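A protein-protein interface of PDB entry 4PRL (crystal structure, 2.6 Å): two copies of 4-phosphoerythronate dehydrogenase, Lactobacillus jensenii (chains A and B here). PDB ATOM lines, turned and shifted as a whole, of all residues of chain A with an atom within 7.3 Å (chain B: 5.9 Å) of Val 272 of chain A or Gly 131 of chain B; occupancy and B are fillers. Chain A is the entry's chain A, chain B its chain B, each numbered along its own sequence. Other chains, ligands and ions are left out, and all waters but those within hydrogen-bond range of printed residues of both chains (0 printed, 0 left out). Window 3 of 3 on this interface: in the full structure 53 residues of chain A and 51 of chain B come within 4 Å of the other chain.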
ATOM      1  N   SER A 266      -3.437 -30.424  24.711  1.00  0.00           N
ATOM      2  CA  SER A 266      -2.904 -29.347  23.885  1.00  0.00           C
ATOM      3  C   SER A 266      -3.856 -28.155  23.729  1.00  0.00           C
ATOM      4  O   SER A 266      -3.412 -27.065  23.406  1.00  0.00           O
ATOM      5  CB  SER A 266      -2.546 -29.870  22.497  1.00  0.00           C
ATOM      6  OG  SER A 266      -3.662 -29.722  21.649  1.00  0.00           O
ATOM      7  N   TYR A 267      -5.153 -28.349  23.928  1.00  0.00           N
ATOM      8  CA  TYR A 267      -6.094 -27.245  23.762  1.00  0.00           C
ATOM      9  C   TYR A 267      -7.196 -27.140  24.784  1.00  0.00           C
ATOM     10  O   TYR A 267      -7.750 -26.063  24.927  1.00  0.00           O
ATOM     11  CB  TYR A 267      -6.705 -27.243  22.363  1.00  0.00           C
ATOM     12  CG  TYR A 267      -7.531 -28.451  22.023  1.00  0.00           C
ATOM     13  CD1 TYR A 267      -6.916 -29.677  21.764  1.00  0.00           C
ATOM     14  CD2 TYR A 267      -8.917 -28.377  21.919  1.00  0.00           C
ATOM     15  CE1 TYR A 267      -7.648 -30.796  21.439  1.00  0.00           C
ATOM     16  CE2 TYR A 267      -9.657 -29.499  21.580  1.00  0.00           C
ATOM     17  CZ  TYR A 267      -9.007 -30.704  21.343  1.00  0.00           C
ATOM     18  OH  TYR A 267      -9.688 -31.845  20.997  1.00  0.00           O
ATOM     19  N   PHE A 268      -7.539 -28.212  25.488  1.00  0.00           N
ATOM     20  CA  PHE A 268      -8.494 -28.086  26.600  1.00  0.00           C
ATOM     21  C   PHE A 268      -7.908 -27.220  27.716  1.00  0.00           C
ATOM     22  O   PHE A 268      -6.743 -27.364  28.068  1.00  0.00           O
ATOM     23  CB  PHE A 268      -8.900 -29.454  27.160  1.00  0.00           C
ATOM     24  CG  PHE A 268     -10.024 -30.119  26.408  1.00  0.00           C
ATOM     25  CD1 PHE A 268     -10.262 -29.851  25.068  1.00  0.00           C
ATOM     26  CD2 PHE A 268     -10.829 -31.045  27.048  1.00  0.00           C
ATOM     27  CE1 PHE A 268     -11.293 -30.490  24.396  1.00  0.00           C
ATOM     28  CE2 PHE A 268     -11.863 -31.687  26.387  1.00  0.00           C
ATOM     29  CZ  PHE A 268     -12.098 -31.410  25.056  1.00  0.00           C
ATOM     30  N   PHE A 269      -8.744 -26.333  28.250  1.00  0.00           N
ATOM     31  CA  PHE A 269      -8.379 -25.348  29.260  1.00  0.00           C
ATOM     32  C   PHE A 269      -7.563 -24.169  28.745  1.00  0.00           C
ATOM     33  O   PHE A 269      -6.825 -23.567  29.515  1.00  0.00           O
ATOM     34  CB  PHE A 269      -7.693 -26.017  30.442  1.00  0.00           C
ATOM     35  CG  PHE A 269      -8.495 -27.120  31.034  1.00  0.00           C
ATOM     36  CD1 PHE A 269      -9.828 -26.903  31.395  1.00  0.00           C
ATOM     37  CD2 PHE A 269      -7.944 -28.362  31.224  1.00  0.00           C
ATOM     38  CE1 PHE A 269     -10.589 -27.911  31.941  1.00  0.00           C
ATOM     39  CE2 PHE A 269      -8.694 -29.380  31.771  1.00  0.00           C
ATOM     40  CZ  PHE A 269     -10.024 -29.156  32.124  1.00  0.00           C
ATOM     41  N   LYS A 270      -7.735 -23.815  27.466  1.00  0.00           N
ATOM     42  CA  LYS A 270      -6.938 -22.768  26.827  1.00  0.00           C
ATOM     43  C   LYS A 270      -7.732 -21.910  25.853  1.00  0.00           C
ATOM     44  O   LYS A 270      -8.850 -22.264  25.450  1.00  0.00           O
ATOM     45  CB  LYS A 270      -5.770 -23.401  26.090  1.00  0.00           C
ATOM     46  CG  LYS A 270      -4.598 -23.661  26.996  1.00  0.00           C
ATOM     47  CD  LYS A 270      -3.774 -24.846  26.547  1.00  0.00           C
ATOM     48  CE  LYS A 270      -2.774 -25.219  27.628  1.00  0.00           C
ATOM     49  NZ  LYS A 270      -1.919 -26.349  27.189  1.00  0.00           N
ATOM     50  N   LYS A 271      -7.153 -20.766  25.484  1.00  0.00           N
ATOM     51  CA  LYS A 271      -7.677 -19.973  24.367  1.00  0.00           C
ATOM     52  C   LYS A 271      -6.657 -20.087  23.261  1.00  0.00           C
ATOM     53  O   LYS A 271      -5.459 -19.895  23.489  1.00  0.00           O
ATOM     54  CB  LYS A 271      -7.919 -18.517  24.750  1.00  0.00           C
ATOM     55  CG  LYS A 271      -8.337 -18.353  26.204  1.00  0.00           C
ATOM     56  CD  LYS A 271      -8.843 -16.960  26.521  1.00  0.00           C
ATOM     57  CE  LYS A 271      -8.436 -16.550  27.929  1.00  0.00           C
ATOM     58  NZ  LYS A 271      -9.350 -15.488  28.414  1.00  0.00           N
ATOM     59  N   VAL A 272      -7.141 -20.434  22.073  1.00  0.00           N
ATOM     60  CA  VAL A 272      -6.285 -20.771  20.970  1.00  0.00           C
ATOM     61  C   VAL A 272      -6.865 -20.339  19.645  1.00  0.00           C
ATOM     62  O   VAL A 272      -8.054 -20.077  19.531  1.00  0.00           O
ATOM     63  CB  VAL A 272      -6.047 -22.281  20.897  1.00  0.00           C
ATOM     64  CG1 VAL A 272      -5.357 -22.766  22.160  1.00  0.00           C
ATOM     65  CG2 VAL A 272      -7.347 -23.042  20.653  1.00  0.00           C
ATOM     66  N   ASP A 273      -5.989 -20.296  18.648  1.00  0.00           N
ATOM     67  CA  ASP A 273      -6.336 -19.937  17.288  1.00  0.00           C
ATOM     68  C   ASP A 273      -6.708 -21.187  16.536  1.00  0.00           C
ATOM     69  O   ASP A 273      -6.148 -22.250  16.796  1.00  0.00           O
ATOM     70  CB  ASP A 273      -5.138 -19.281  16.603  1.00  0.00           C
ATOM     71  CG  ASP A 273      -4.656 -18.060  17.345  1.00  0.00           C
ATOM     72  OD1 ASP A 273      -5.501 -17.206  17.667  1.00  0.00           O
ATOM     73  OD2 ASP A 273      -3.445 -17.949  17.623  1.00  0.00           O
ATOM     74  N   ASP A 274      -7.637 -21.048  15.591  1.00  0.00           N
ATOM     75  CA  ASP A 274      -8.035 -22.139  14.695  1.00  0.00           C
ATOM     76  C   ASP A 274      -6.912 -23.137  14.387  1.00  0.00           C
ATOM     77  O   ASP A 274      -7.101 -24.352  14.478  1.00  0.00           O
ATOM     78  CB  ASP A 274      -8.562 -21.560  13.373  1.00  0.00           C
ATOM     79  CG  ASP A 274     -10.072 -21.464  13.334  1.00  0.00           C
ATOM     80  OD1 ASP A 274     -10.737 -21.975  14.272  1.00  0.00           O
ATOM     81  OD2 ASP A 274     -10.592 -20.880  12.351  1.00  0.00           O
ATOM     82  N   ALA A 275      -5.754 -22.605  14.020  1.00  0.00           N
ATOM     83  CA  ALA A 275      -4.613 -23.404  13.632  1.00  0.00           C
ATOM     84  C   ALA A 275      -4.121 -24.338  14.723  1.00  0.00           C
ATOM     85  O   ALA A 275      -3.465 -25.334  14.419  1.00  0.00           O
ATOM     86  CB  ALA A 275      -3.484 -22.484  13.249  1.00  0.00           C
ATOM     87  N   GLN A 276      -4.404 -24.001  15.983  1.00  0.00           N
ATOM     88  CA  GLN A 276      -3.934 -24.777  17.135  1.00  0.00           C
ATOM     89  C   GLN A 276      -4.928 -25.860  17.589  1.00  0.00           C
ATOM     90  O   GLN A 276      -4.635 -26.610  18.521  1.00  0.00           O
ATOM     91  CB  GLN A 276      -3.665 -23.863  18.328  1.00  0.00           C
ATOM     92  CG  GLN A 276      -2.997 -22.549  17.998  1.00  0.00           C
ATOM     93  CD  GLN A 276      -2.549 -21.805  19.237  1.00  0.00           C
ATOM     94  OE1 GLN A 276      -3.168 -20.820  19.637  1.00  0.00           O
ATOM     95  NE2 GLN A 276      -1.470 -22.285  19.859  1.00  0.00           N
ATOM     96  N   ILE A 277      -6.104 -25.898  16.972  1.00  0.00           N
ATOM     97  CA  ILE A 277      -7.127 -26.857  17.320  1.00  0.00           C
ATOM     98  C   ILE A 277      -6.935 -28.015  16.371  1.00  0.00           C
ATOM     99  O   ILE A 277      -6.856 -27.798  15.168  1.00  0.00           O
ATOM    100  CB  ILE A 277      -8.540 -26.273  17.121  1.00  0.00           C
ATOM    101  CG1 ILE A 277      -8.719 -25.009  17.949  1.00  0.00           C
ATOM    102  CG2 ILE A 277      -9.605 -27.284  17.526  1.00  0.00           C
ATOM    103  CD1 ILE A 277     -10.021 -24.286  17.676  1.00  0.00           C
ATOM    104  N   PRO A 278      -6.875 -29.251  16.898  1.00  0.00           N
ATOM    105  CA  PRO A 278      -6.660 -30.409  16.011  1.00  0.00           C
ATOM    106  C   PRO A 278      -7.845 -30.699  15.082  1.00  0.00           C
ATOM    107  O   PRO A 278      -8.979 -30.254  15.327  1.00  0.00           O
ATOM    108  CB  PRO A 278      -6.424 -31.572  16.982  1.00  0.00           C
ATOM    109  CG  PRO A 278      -7.013 -31.143  18.287  1.00  0.00           C
ATOM    110  CD  PRO A 278      -7.030 -29.639  18.317  1.00  0.00           C
ATOM    111  N   ALA B 126     -20.245 -22.385  22.103  1.00  0.00           N
ATOM    112  CA  ALA B 126     -20.078 -21.064  21.533  1.00  0.00           C
ATOM    113  C   ALA B 126     -18.705 -20.509  21.905  1.00  0.00           C
ATOM    114  O   ALA B 126     -18.011 -19.921  21.062  1.00  0.00           O
ATOM    115  CB  ALA B 126     -21.182 -20.155  22.017  1.00  0.00           C
ATOM    116  N   ASN B 127     -18.330 -20.714  23.168  1.00  0.00           N
ATOM    117  CA  ASN B 127     -16.984 -20.424  23.650  1.00  0.00           C
ATOM    118  C   ASN B 127     -15.926 -21.169  22.845  1.00  0.00           C
ATOM    119  O   ASN B 127     -14.915 -20.591  22.490  1.00  0.00           O
ATOM    120  CB  ASN B 127     -16.831 -20.794  25.143  1.00  0.00           C
ATOM    121  CG  ASN B 127     -16.968 -19.599  26.079  1.00  0.00           C
ATOM    122  OD1 ASN B 127     -17.511 -18.562  25.715  1.00  0.00           O
ATOM    123  ND2 ASN B 127     -16.497 -19.760  27.308  1.00  0.00           N
ATOM    124  N   MET B 128     -16.171 -22.448  22.578  1.00  0.00           N
ATOM    125  CA  MET B 128     -15.214 -23.313  21.886  1.00  0.00           C
ATOM    126  C   MET B 128     -15.064 -22.971  20.406  1.00  0.00           C
ATOM    127  O   MET B 128     -13.933 -22.942  19.887  1.00  0.00           O
ATOM    128  CB  MET B 128     -15.597 -24.795  22.060  1.00  0.00           C
ATOM    129  CG  MET B 128     -15.312 -25.292  23.469  1.00  0.00           C
ATOM    130  SD  MET B 128     -16.259 -26.706  24.065  1.00  0.00           S
ATOM    131  CE  MET B 128     -15.062 -28.013  23.938  1.00  0.00           C
ATOM    132  N   ASP B 129     -16.192 -22.706  19.738  1.00  0.00           N
ATOM    133  CA  ASP B 129     -16.197 -22.268  18.330  1.00  0.00           C
ATOM    134  C   ASP B 129     -15.265 -21.051  18.124  1.00  0.00           C
ATOM    135  O   ASP B 129     -14.771 -20.833  17.040  1.00  0.00           O
ATOM    136  CB  ASP B 129     -17.623 -21.892  17.852  1.00  0.00           C
ATOM    137  CG  ASP B 129     -18.563 -23.104  17.662  1.00  0.00           C
ATOM    138  OD1 ASP B 129     -18.119 -24.263  17.716  1.00  0.00           O
ATOM    139  OD2 ASP B 129     -19.776 -22.886  17.456  1.00  0.00           O
ATOM    140  N   LYS B 130     -15.050 -20.254  19.161  1.00  0.00           N
ATOM    141  CA  LYS B 130     -14.198 -19.083  19.080  1.00  0.00           C
ATOM    142  C   LYS B 130     -12.800 -19.350  19.637  1.00  0.00           C
ATOM    143  O   LYS B 130     -11.984 -18.425  19.717  1.00  0.00           O
ATOM    144  CB  LYS B 130     -14.848 -17.923  19.846  1.00  0.00           C
ATOM    145  CG  LYS B 130     -16.177 -17.462  19.255  1.00  0.00           C
ATOM    146  CD  LYS B 130     -17.117 -16.844  20.288  1.00  0.00           C
ATOM    147  CE  LYS B 130     -16.615 -15.504  20.798  1.00  0.00           C
ATOM    148  NZ  LYS B 130     -17.724 -14.706  21.393  1.00  0.00           N
ATOM    149  N   GLY B 131     -12.519 -20.597  20.030  1.00  0.00           N
ATOM    150  CA  GLY B 131     -11.189 -20.978  20.517  1.00  0.00           C
ATOM    151  C   GLY B 131     -11.026 -21.025  22.021  1.00  0.00           C
ATOM    152  O   GLY B 131      -9.930 -21.305  22.528  1.00  0.00           O
ATOM    153  N   ASP B 132     -12.103 -20.756  22.751  1.00  0.00           N
ATOM    154  CA  ASP B 132     -12.050 -20.765  24.207  1.00  0.00           C
ATOM    155  C   ASP B 132     -12.484 -22.127  24.807  1.00  0.00           C
ATOM    156  O   ASP B 132     -13.688 -22.477  24.831  1.00  0.00           O
ATOM    157  CB  ASP B 132     -12.902 -19.626  24.753  1.00  0.00           C
ATOM    158  CG  ASP B 132     -12.593 -19.312  26.196  1.00  0.00           C
ATOM    159  OD1 ASP B 132     -11.966 -20.153  26.905  1.00  0.00           O
ATOM    160  OD2 ASP B 132     -12.993 -18.208  26.619  1.00  0.00           O
ATOM    161  N   PHE B 133     -11.485 -22.871  25.303  1.00  0.00           N
ATOM    162  CA  PHE B 133     -11.696 -24.193  25.934  1.00  0.00           C
ATOM    163  C   PHE B 133     -11.463 -24.133  27.433  1.00  0.00           C
ATOM    164  O   PHE B 133     -11.155 -25.136  28.075  1.00  0.00           O
ATOM    165  CB  PHE B 133     -10.808 -25.263  25.288  1.00  0.00           C
ATOM    166  CG  PHE B 133     -11.072 -25.453  23.822  1.00  0.00           C
ATOM    167  CD1 PHE B 133     -10.497 -24.605  22.885  1.00  0.00           C
ATOM    168  CD2 PHE B 133     -11.910 -26.466  23.375  1.00  0.00           C
ATOM    169  CE1 PHE B 133     -10.749 -24.759  21.531  1.00  0.00           C
ATOM    170  CE2 PHE B 133     -12.152 -26.633  22.021  1.00  0.00           C
ATOM    171  CZ  PHE B 133     -11.572 -25.777  21.097  1.00  0.00           C
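O of Phe 133 of chain B is in hydrogen-bond range of N of Phe 269 of chain A, at 2.7 Å. N of Phe 133 of chain B lies within hydrogen-bond range of O of Lys 270 of chain A, 2.7 Å away. The backbone carbonyl oxygen of Gly 131 of chain B is in hydrogen-bond range of the backbone NH of Val 272 of chain A (3.0 Å). The backbone carbonyl oxygen (O) of Lys 270 of chain A sits close to the backbone carbonyl oxygen (O) of Gly 131 of chain B (3.3 Å).
O of Asn 127 of chain B is in hydrogen-bond range of N of Asp 132 of chain B (2.8 Å).
Among the printed residues, merely in contact across the chains: Tyr 267 of chain A with Phe 133 of chain B (3.2 Å), Lys 271 of chain A with Gly 131 of chain B (3.2 Å), Lys 270 of chain A with Asp 132 of chain B (3.7 Å), Phe 268 of chain A with Phe 133 of chain B (3.9 Å), Val 272 of chain A with Phe 133 of chain B (3.9 Å) and Ile 277 of chain A with Phe 133 of chain B (3.95 Å).
Of the printed residues of chain B, Lys 270 of chain A touches Gly 131 (3.3 Å), Asp 132 (3.7 Å) and Phe 133 (2.7 Å). Of the printed residues of chain B, Phe 269 of chain A touches Phe 133. Printed residues of chain B within 4 Å of Phe 268 of chain A: Phe 133 (3.9 Å). Ser 266 of chain A touches none of the printed residues of chain B. Ala 126 of chain B touches none of the printed residues of chain A. The nearest residue of chain B that does not touch Val 272 of chain A is Lys 130 of chain B (4.3 Å). The nearest residue of chain A that does not touch Gly 131 of chain B is Ile 277 of chain A (4.5 Å). The nearest printed residue of chain B that does not touch Phe 269 of chain A is Asp 132 of chain B (6.2 Å).
Hydrophobic or aromatic side chains of chain B that line the printed part of chain A: Phe 133. Printed residues of chain A that touch a printed residue of chain B: Tyr 267, Phe 268, Phe 269, Lys 270, Lys 271, Val 272 and Ile 277. Hydrophobic or aromatic side chains of chain A within 4 Å of the printed part of chain B: Tyr 267, Phe 269, Val 272 and Ile 277. Among the printed residues, no Asp or Glu carboxylate lies within 4 Å of a Lys or Arg side-chain nitrogen of the other chain.
No position is printed for both chains. Of the 10 pairs that touch across the chains among the printed residues, none has its exchanged pair printed and touching as well.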
